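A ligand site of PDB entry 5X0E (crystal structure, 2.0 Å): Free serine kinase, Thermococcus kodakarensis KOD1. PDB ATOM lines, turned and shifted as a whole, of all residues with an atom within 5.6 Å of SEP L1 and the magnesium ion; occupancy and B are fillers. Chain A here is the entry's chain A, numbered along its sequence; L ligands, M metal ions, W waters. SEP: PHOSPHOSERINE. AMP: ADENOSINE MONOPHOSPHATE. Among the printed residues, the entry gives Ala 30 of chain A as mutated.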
ATOM      1  N   GLU A   4      14.868  30.864   6.927  1.00  0.00           N
ATOM      2  CA  GLU A   4      13.401  30.957   6.808  1.00  0.00           C
ATOM      3  C   GLU A   4      12.701  31.272   8.139  1.00  0.00           C
ATOM      4  O   GLU A   4      13.089  30.769   9.194  1.00  0.00           O
ATOM      5  CB  GLU A   4      12.820  29.675   6.196  1.00  0.00           C
ATOM      6  CG  GLU A   4      13.254  29.432   4.739  1.00  0.00           C
ATOM      7  CD  GLU A   4      13.134  27.972   4.311  1.00  0.00           C
ATOM      8  OE1 GLU A   4      13.158  27.071   5.169  1.00  0.00           O
ATOM      9  OE2 GLU A   4      13.025  27.719   3.097  1.00  0.00           O
ATOM     10  N   HIS A  29      15.922  22.467  -8.774  1.00  0.00           N
ATOM     11  CA  HIS A  29      15.187  23.505  -9.501  1.00  0.00           C
ATOM     12  C   HIS A  29      15.449  24.957  -9.097  1.00  0.00           C
ATOM     13  O   HIS A  29      14.869  25.862  -9.675  1.00  0.00           O
ATOM     14  CB  HIS A  29      13.679  23.167  -9.483  1.00  0.00           C
ATOM     15  CG  HIS A  29      12.972  23.444  -8.201  1.00  0.00           C
ATOM     16  ND1 HIS A  29      12.730  22.463  -7.265  1.00  0.00           N
ATOM     17  CD2 HIS A  29      12.388  24.567  -7.723  1.00  0.00           C
ATOM     18  CE1 HIS A  29      12.052  22.973  -6.256  1.00  0.00           C
ATOM     19  NE2 HIS A  29      11.831  24.249  -6.502  1.00  0.00           N
ATOM     20  N   ALA A  30      16.370  25.184  -8.158  1.00  0.00           N
ATOM     21  CA  ALA A  30      16.598  26.525  -7.576  1.00  0.00           C
ATOM     22  C   ALA A  30      18.057  26.723  -7.186  1.00  0.00           C
ATOM     23  O   ALA A  30      18.787  25.770  -6.923  1.00  0.00           O
ATOM     24  CB  ALA A  30      15.699  26.750  -6.369  1.00  0.00           C
ATOM     25  N   GLN A  31      18.445  27.999  -7.148  1.00  0.00           N
ATOM     26  CA  GLN A  31      19.722  28.438  -6.599  1.00  0.00           C
ATOM     27  C   GLN A  31      19.772  28.380  -5.065  1.00  0.00           C
ATOM     28  O   GLN A  31      18.755  28.136  -4.403  1.00  0.00           O
ATOM     29  CB  GLN A  31      20.011  29.853  -7.073  1.00  0.00           C
ATOM     30  CG  GLN A  31      20.331  29.937  -8.553  1.00  0.00           C
ATOM     31  CD  GLN A  31      20.412  31.362  -9.037  1.00  0.00           C
ATOM     32  OE1 GLN A  31      19.659  32.222  -8.604  1.00  0.00           O
ATOM     33  NE2 GLN A  31      21.327  31.606  -9.958  1.00  0.00           N
ATOM     34  N   GLU A  36      22.108  29.916   4.364  1.00  0.00           N
ATOM     35  CA  GLU A  36      21.309  28.699   4.531  1.00  0.00           C
ATOM     36  C   GLU A  36      22.189  27.439   4.341  1.00  0.00           C
ATOM     37  O   GLU A  36      22.105  26.484   5.122  1.00  0.00           O
ATOM     38  CB  GLU A  36      20.137  28.699   3.553  1.00  0.00           C
ATOM     39  CG  GLU A  36      19.143  27.552   3.671  1.00  0.00           C
ATOM     40  CD  GLU A  36      18.106  27.744   4.760  1.00  0.00           C
ATOM     41  OE1 GLU A  36      16.937  27.373   4.517  1.00  0.00           O
ATOM     42  OE2 GLU A  36      18.438  28.265   5.854  1.00  0.00           O
ATOM     43  N   ILE A  67      14.333  17.803  -6.771  1.00  0.00           N
ATOM     44  CA  ILE A  67      14.399  18.272  -5.387  1.00  0.00           C
ATOM     45  C   ILE A  67      13.193  19.184  -5.207  1.00  0.00           C
ATOM     46  O   ILE A  67      13.117  20.241  -5.814  1.00  0.00           O
ATOM     47  CB  ILE A  67      15.710  19.012  -5.063  1.00  0.00           C
ATOM     48  CG1 ILE A  67      16.896  18.055  -5.218  1.00  0.00           C
ATOM     49  CG2 ILE A  67      15.669  19.565  -3.646  1.00  0.00           C
ATOM     50  CD1 ILE A  67      18.255  18.720  -5.183  1.00  0.00           C
ATOM     51  N   VAL A  68      12.217  18.721  -4.423  1.00  0.00           N
ATOM     52  CA  VAL A  68      11.008  19.485  -4.146  1.00  0.00           C
ATOM     53  C   VAL A  68      11.360  20.480  -3.030  1.00  0.00           C
ATOM     54  O   VAL A  68      11.084  21.669  -3.160  1.00  0.00           O
ATOM     55  CB  VAL A  68       9.836  18.553  -3.756  1.00  0.00           C
ATOM     56  CG1 VAL A  68       8.624  19.331  -3.266  1.00  0.00           C
ATOM     57  CG2 VAL A  68       9.436  17.671  -4.941  1.00  0.00           C
ATOM     58  N   ASP A  69      11.962  19.952  -1.964  1.00  0.00           N
ATOM     59  CA  ASP A  69      12.500  20.736  -0.872  1.00  0.00           C
ATOM     60  C   ASP A  69      13.786  20.083  -0.391  1.00  0.00           C
ATOM     61  O   ASP A  69      13.807  18.856  -0.186  1.00  0.00           O
ATOM     62  CB  ASP A  69      11.484  20.771   0.268  1.00  0.00           C
ATOM     63  CG  ASP A  69      11.958  21.580   1.468  1.00  0.00           C
ATOM     64  OD1 ASP A  69      12.794  22.516   1.352  1.00  0.00           O
ATOM     65  OD2 ASP A  69      11.486  21.268   2.586  1.00  0.00           O
ATOM     66  N   GLY A  70      14.846  20.875  -0.194  1.00  0.00           N
ATOM     67  CA  GLY A  70      16.141  20.324   0.190  1.00  0.00           C
ATOM     68  C   GLY A  70      17.371  20.673  -0.642  1.00  0.00           C
ATOM     69  O   GLY A  70      18.325  19.904  -0.653  1.00  0.00           O
ATOM     70  N   HIS A  71      17.396  21.831  -1.278  1.00  0.00           N
ATOM     71  CA  HIS A  71      18.550  22.240  -2.110  1.00  0.00           C
ATOM     72  C   HIS A  71      19.850  22.397  -1.336  1.00  0.00           C
ATOM     73  O   HIS A  71      20.919  22.052  -1.841  1.00  0.00           O
ATOM     74  CB  HIS A  71      18.259  23.537  -2.846  1.00  0.00           C
ATOM     75  CG  HIS A  71      17.256  23.370  -3.933  1.00  0.00           C
ATOM     76  ND1 HIS A  71      15.899  23.378  -3.692  1.00  0.00           N
ATOM     77  CD2 HIS A  71      17.411  23.085  -5.242  1.00  0.00           C
ATOM     78  CE1 HIS A  71      15.260  23.146  -4.821  1.00  0.00           C
ATOM     79  NE2 HIS A  71      16.149  22.961  -5.764  1.00  0.00           N
ATOM     80  N   HIS A  72      19.741  22.900  -0.110  1.00  0.00           N
ATOM     81  CA  HIS A  72      20.892  23.207   0.707  1.00  0.00           C
ATOM     82  C   HIS A  72      21.406  21.973   1.386  1.00  0.00           C
ATOM     83  O   HIS A  72      22.624  21.814   1.529  1.00  0.00           O
ATOM     84  CB  HIS A  72      20.545  24.291   1.713  1.00  0.00           C
ATOM     85  CG  HIS A  72      20.184  25.570   1.057  1.00  0.00           C
ATOM     86  ND1 HIS A  72      18.951  25.804   0.494  1.00  0.00           N
ATOM     87  CD2 HIS A  72      20.942  26.659   0.769  1.00  0.00           C
ATOM     88  CE1 HIS A  72      18.944  26.999  -0.061  1.00  0.00           C
ATOM     89  NE2 HIS A  72      20.141  27.534   0.089  1.00  0.00           N
ATOM     90  N   ARG A  73      20.487  21.126   1.837  1.00  0.00           N
ATOM     91  CA  ARG A  73      20.867  19.795   2.329  1.00  0.00           C
ATOM     92  C   ARG A  73      21.610  19.016   1.225  1.00  0.00           C
ATOM     93  O   ARG A  73      22.668  18.430   1.461  1.00  0.00           O
ATOM     94  CB  ARG A  73      19.640  19.020   2.836  1.00  0.00           C
ATOM     95  CG  ARG A  73      19.251  19.395   4.256  1.00  0.00           C
ATOM     96  CD  ARG A  73      17.863  18.910   4.605  1.00  0.00           C
ATOM     97  NE  ARG A  73      16.826  19.693   3.941  1.00  0.00           N
ATOM     98  CZ  ARG A  73      15.544  19.366   3.882  1.00  0.00           C
ATOM     99  NH1 ARG A  73      15.093  18.224   4.426  1.00  0.00           N
ATOM    100  NH2 ARG A  73      14.687  20.172   3.253  1.00  0.00           N
ATOM    101  N   TRP A 102       8.405  31.750  -1.231  1.00  0.00           N
ATOM    102  CA  TRP A 102       9.045  32.403  -0.090  1.00  0.00           C
ATOM    103  C   TRP A 102       9.407  33.806  -0.537  1.00  0.00           C
ATOM    104  O   TRP A 102       9.932  33.977  -1.651  1.00  0.00           O
ATOM    105  CB  TRP A 102      10.337  31.692   0.313  1.00  0.00           C
ATOM    106  CG  TRP A 102      10.158  30.307   0.844  1.00  0.00           C
ATOM    107  CD1 TRP A 102      10.232  29.143   0.143  1.00  0.00           C
ATOM    108  CD2 TRP A 102       9.896  29.940   2.202  1.00  0.00           C
ATOM    109  NE1 TRP A 102      10.013  28.075   0.964  1.00  0.00           N
ATOM    110  CE2 TRP A 102       9.810  28.527   2.239  1.00  0.00           C
ATOM    111  CE3 TRP A 102       9.719  30.652   3.389  1.00  0.00           C
ATOM    112  CZ2 TRP A 102       9.552  27.817   3.426  1.00  0.00           C
ATOM    113  CZ3 TRP A 102       9.483  29.943   4.581  1.00  0.00           C
ATOM    114  CH2 TRP A 102       9.384  28.539   4.569  1.00  0.00           C
ATOM    115  N   LYS A 221      14.695  29.795  -3.193  1.00  0.00           N
ATOM    116  CA  LYS A 221      13.459  29.755  -2.410  1.00  0.00           C
ATOM    117  C   LYS A 221      12.207  30.114  -3.201  1.00  0.00           C
ATOM    118  O   LYS A 221      11.226  30.585  -2.624  1.00  0.00           O
ATOM    119  CB  LYS A 221      13.566  30.654  -1.161  1.00  0.00           C
ATOM    120  CG  LYS A 221      14.757  30.370  -0.272  1.00  0.00           C
ATOM    121  CD  LYS A 221      14.679  28.981   0.326  1.00  0.00           C
ATOM    122  CE  LYS A 221      15.740  28.753   1.394  1.00  0.00           C
ATOM    123  NZ  LYS A 221      15.591  27.418   2.056  1.00  0.00           N
ATOM    124  N   THR A 222      12.225  29.863  -4.501  1.00  0.00           N
ATOM    125  CA  THR A 222      11.129  30.252  -5.390  1.00  0.00           C
ATOM    126  C   THR A 222       9.858  29.447  -5.105  1.00  0.00           C
ATOM    127  O   THR A 222       8.763  29.987  -5.171  1.00  0.00           O
ATOM    128  CB  THR A 222      11.526  30.143  -6.881  1.00  0.00           C
ATOM    129  OG1 THR A 222      12.496  31.145  -7.200  1.00  0.00           O
ATOM    130  CG2 THR A 222      10.302  30.294  -7.800  1.00  0.00           C
ATOM    131  N   THR A 223      10.015  28.172  -4.773  1.00  0.00           N
ATOM    132  CA  THR A 223       8.897  27.320  -4.398  1.00  0.00           C
ATOM    133  C   THR A 223       8.824  27.106  -2.888  1.00  0.00           C
ATOM    134  O   THR A 223       9.845  26.902  -2.237  1.00  0.00           O
ATOM    135  CB  THR A 223       9.004  25.929  -5.041  1.00  0.00           C
ATOM    136  OG1 THR A 223      10.214  25.288  -4.615  1.00  0.00           O
ATOM    137  CG2 THR A 223       8.952  25.986  -6.589  1.00  0.00           C
ATOM    138  N   ARG A 224       7.611  27.133  -2.352  1.00  0.00           N
ATOM    139  CA  ARG A 224       7.316  26.724  -0.996  1.00  0.00           C
ATOM    140  C   ARG A 224       6.235  25.662  -1.126  1.00  0.00           C
ATOM    141  O   ARG A 224       5.041  25.962  -1.246  1.00  0.00           O
ATOM    142  CB  ARG A 224       6.809  27.898  -0.151  1.00  0.00           C
ATOM    143  CG  ARG A 224       6.448  27.521   1.291  1.00  0.00           C
ATOM    144  CD  ARG A 224       6.279  28.765   2.144  1.00  0.00           C
ATOM    145  NE  ARG A 224       5.068  29.508   1.808  1.00  0.00           N
ATOM    146  CZ  ARG A 224       3.838  29.209   2.227  1.00  0.00           C
ATOM    147  NH1 ARG A 224       3.607  28.132   2.971  1.00  0.00           N
ATOM    148  NH2 ARG A 224       2.798  29.967   1.878  1.00  0.00           N
ATOM    149  N   HIS A 225       6.669  24.412  -1.106  1.00  0.00           N
ATOM    150  CA  HIS A 225       5.780  23.286  -1.237  1.00  0.00           C
ATOM    151  C   HIS A 225       5.171  22.931   0.091  1.00  0.00           C
ATOM    152  O   HIS A 225       5.874  22.901   1.091  1.00  0.00           O
ATOM    153  CB  HIS A 225       6.548  22.098  -1.771  1.00  0.00           C
ATOM    154  CG  HIS A 225       6.991  22.253  -3.195  1.00  0.00           C
ATOM    155  ND1 HIS A 225       8.216  22.750  -3.532  1.00  0.00           N
ATOM    156  CD2 HIS A 225       6.361  21.957  -4.353  1.00  0.00           C
ATOM    157  CE1 HIS A 225       8.349  22.744  -4.852  1.00  0.00           C
ATOM    158  NE2 HIS A 225       7.219  22.293  -5.375  1.00  0.00           N
HETATM  159  N   SEP L   1      11.720  24.359  -2.566  1.00  0.00           N
HETATM  160  CA  SEP L   1      11.767  24.630  -1.103  1.00  0.00           C
HETATM  161  CB  SEP L   1      12.426  25.974  -0.815  1.00  0.00           C
HETATM  162  OG  SEP L   1      13.762  25.921  -1.302  1.00  0.00           O
HETATM  163  C   SEP L   1      10.375  24.536  -0.528  1.00  0.00           C
HETATM  164  O   SEP L   1      10.098  25.058   0.555  1.00  0.00           O
HETATM  165  OXT SEP L   1       9.500  23.916  -1.135  1.00  0.00           O
HETATM  166  P   SEP L   1      14.911  25.082  -0.522  1.00  0.00           P
HETATM  167  O1P SEP L   1      14.399  25.014   0.902  1.00  0.00           O
HETATM  168  O2P SEP L   1      16.133  25.925  -0.781  1.00  0.00           O
HETATM  169  O3P SEP L   1      14.935  23.762  -1.249  1.00  0.00           O
HETATM  170  P   AMP L   2      17.000  23.086   2.380  1.00  0.00           P
HETATM  171  O1P AMP L   2      17.863  21.856   2.605  1.00  0.00           O
HETATM  172  O2P AMP L   2      17.287  23.850   1.110  1.00  0.00           O
HETATM  173  O3P AMP L   2      15.558  22.803   2.645  1.00  0.00           O
HETATM  174  O5' AMP L   2      17.472  24.115   3.532  1.00  0.00           O
HETATM  175  C5' AMP L   2      18.133  23.703   4.723  1.00  0.00           C
HETATM  176  C4' AMP L   2      17.238  22.814   5.585  1.00  0.00           C
HETATM  177  O4' AMP L   2      18.060  22.046   6.445  1.00  0.00           O
HETATM  178  C3' AMP L   2      16.263  23.561   6.490  1.00  0.00           C
HETATM  179  O3' AMP L   2      14.971  23.007   6.294  1.00  0.00           O
HETATM  180  C2' AMP L   2      16.748  23.286   7.898  1.00  0.00           C
HETATM  181  O2' AMP L   2      15.652  23.182   8.794  1.00  0.00           O
HETATM  182  C1' AMP L   2      17.425  21.939   7.720  1.00  0.00           C
HETATM  183  N9  AMP L   2      18.424  21.497   8.722  1.00  0.00           N
HETATM  184  C8  AMP L   2      19.160  22.211   9.607  1.00  0.00           C
HETATM  185  N7  AMP L   2      19.954  21.400  10.343  1.00  0.00           N
HETATM  186  C5  AMP L   2      19.745  20.143   9.892  1.00  0.00           C
HETATM  187  C6  AMP L   2      20.238  18.798  10.214  1.00  0.00           C
HETATM  188  N6  AMP L   2      21.167  18.632  11.168  1.00  0.00           N
HETATM  189  N1  AMP L   2      19.746  17.749   9.500  1.00  0.00           N
HETATM  190  C2  AMP L   2      18.808  17.895   8.526  1.00  0.00           C
HETATM  191  N3  AMP L   2      18.314  19.092   8.208  1.00  0.00           N
HETATM  192  C4  AMP L   2      18.736  20.223   8.836  1.00  0.00           C
HETATM  193 MG    MG M   1      13.832  23.937   2.470  1.00  0.00          MG
HETATM  194  O   HOH W   1       7.995  24.055   2.098  1.00  0.00           O
HETATM  195  O   HOH W   2      16.153  27.510  -2.979  1.00  0.00           O
HETATM  196  O   HOH W   3      14.784  25.179   3.872  1.00  0.00           O
HETATM  197  O   HOH W   4      13.318  26.470  -4.103  1.00  0.00           O
HETATM  198  O   HOH W   5      13.003  22.867   4.218  1.00  0.00           O
HETATM  199  O   HOH W   6      12.116  25.305   2.693  1.00  0.00           O
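The magnesium ion is bound by an oxygen (O1P) of SEP L1, an oxygen (O3P) of AMP L2, the side-chain carboxylate of Asp 69, water W3, water W6 and water W5.
Residues that only touch SEP L1: Arg 224 (3.6 Å), Glu 4 (3.7 Å) and His 29 (3.9 Å).
Hydrophobic or aromatic side chains that line SEP L1: His 29, His 71, His 72, Trp 102 and His 225.
The nearest printed residue that does not touch SEP L1 is Ile 67 (4.9 Å).
Glu 4 touches the magnesium ion.
Arg 73 touches the magnesium ion (NH2 to MG, 3.9 Å).
Lys 221 touches the magnesium ion.
Within 4 Å of the magnesium ion: Glu 4, Asp 69, Arg 73 and Lys 221.
Along chain A the residues within 4 Å of the magnesium ion span positions 4 to 221.
The guanidinium group of Arg 73 lies within salt-bridge range of the side-chain carboxylate of Asp 69.
A ring nitrogen (NE2) of His 71 sits at hydrogen-bond distance from the backbone NH of Ala 30, 3.3 Å away.
The side-chain hydroxyl (OG1) of Thr 223 lies close to a ring nitrogen (ND1) of His 225.
O of Thr 223 sits close to NE1 of Trp 102.
A ring nitrogen (NE2) of His 29 lies within hydrogen-bond range of the side-chain hydroxyl of Thr 223 (2.7 Å).
O of Lys 221 lies close to N of Trp 102 (3.4 Å).
OE1 of Glu 36 lies within salt-bridge range of NZ of Lys 221, 2.8 Å away.
A ring nitrogen (ND1) of His 29 sits at hydrogen-bond distance from the backbone carbonyl oxygen (O) of Ile 67.
The backbone NH (N) of His 71 sits at hydrogen-bond distance from an oxygen (O3P) of SEP L1, 3.1 Å away.
A ring nitrogen (ND1) of His 71 is in hydrogen-bond range of an oxygen (O3P) of SEP L1 (2.7 Å).
The backbone carbonyl oxygen of Thr 223 sits close to a nitrogen (N) of SEP L1 (3.2 Å).
N of SEP L1 is in hydrogen-bond range of OG1 of Thr 223 (2.7 Å).
The backbone carbonyl oxygen (O) of Val 68 sits at hydrogen-bond distance from a nitrogen (N) of SEP L1.
N of His 225 sits at hydrogen-bond distance from OXT of SEP L1.
An oxygen (OXT) of SEP L1 lies within hydrogen-bond range of a ring nitrogen (ND1) of His 225, 3.0 Å away.
NZ of Lys 221 is in salt-bridge range of O2P of SEP L1.
The indole nitrogen (NE1) of Trp 102 is in hydrogen-bond range of an oxygen (O) of SEP L1, 3.0 Å away.
The backbone NH of Gly 70 is in hydrogen-bond range of an oxygen (O3P) of SEP L1, 3.1 Å away.
ND1 of His 72 sits close to O2P of SEP L1 (3.1 Å).
N of His 71 lies within hydrogen-bond range of O2P of AMP L2 (3.1 Å).
The backbone NH (N) of His 72 lies within hydrogen-bond range of an oxygen (O2P) of AMP L2, 2.9 Å away.
A ring nitrogen (ND1) of His 72 sits at hydrogen-bond distance from an oxygen (O2P) of AMP L2, 2.6 Å away.
N of Arg 73 is in hydrogen-bond range of O1P of AMP L2 (2.8 Å).
NE of Arg 73 is in salt-bridge range of O1P of AMP L2 (2.7 Å).
Water W5 lies within hydrogen-bond range of the side-chain carboxylate (OD2) of Asp 69 (2.7 Å), an oxygen (O3') of AMP L2 (2.9 Å) and the guanidinium group (NH2) of Arg 73 (3.3 Å).
Water W6 lies within hydrogen-bond range of the side-chain carboxylate of Glu 4 (2.6 Å) and an oxygen (O) of SEP L1 (3.0 Å).
Water W2 lies within hydrogen-bond range of an oxygen (O2P) of SEP L1 (2.7 Å), the backbone NH of Lys 221 (2.7 Å) and the backbone carbonyl oxygen of Gln 31 (3.0 Å).
Water W1 lies within hydrogen-bond range of the backbone carbonyl oxygen (O) of His 225 and an oxygen (O) of SEP L1.
Water W4 lies within hydrogen-bond range of OG of SEP L1 (2.9 Å) and OG1 of Thr 223 (3.4 Å).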
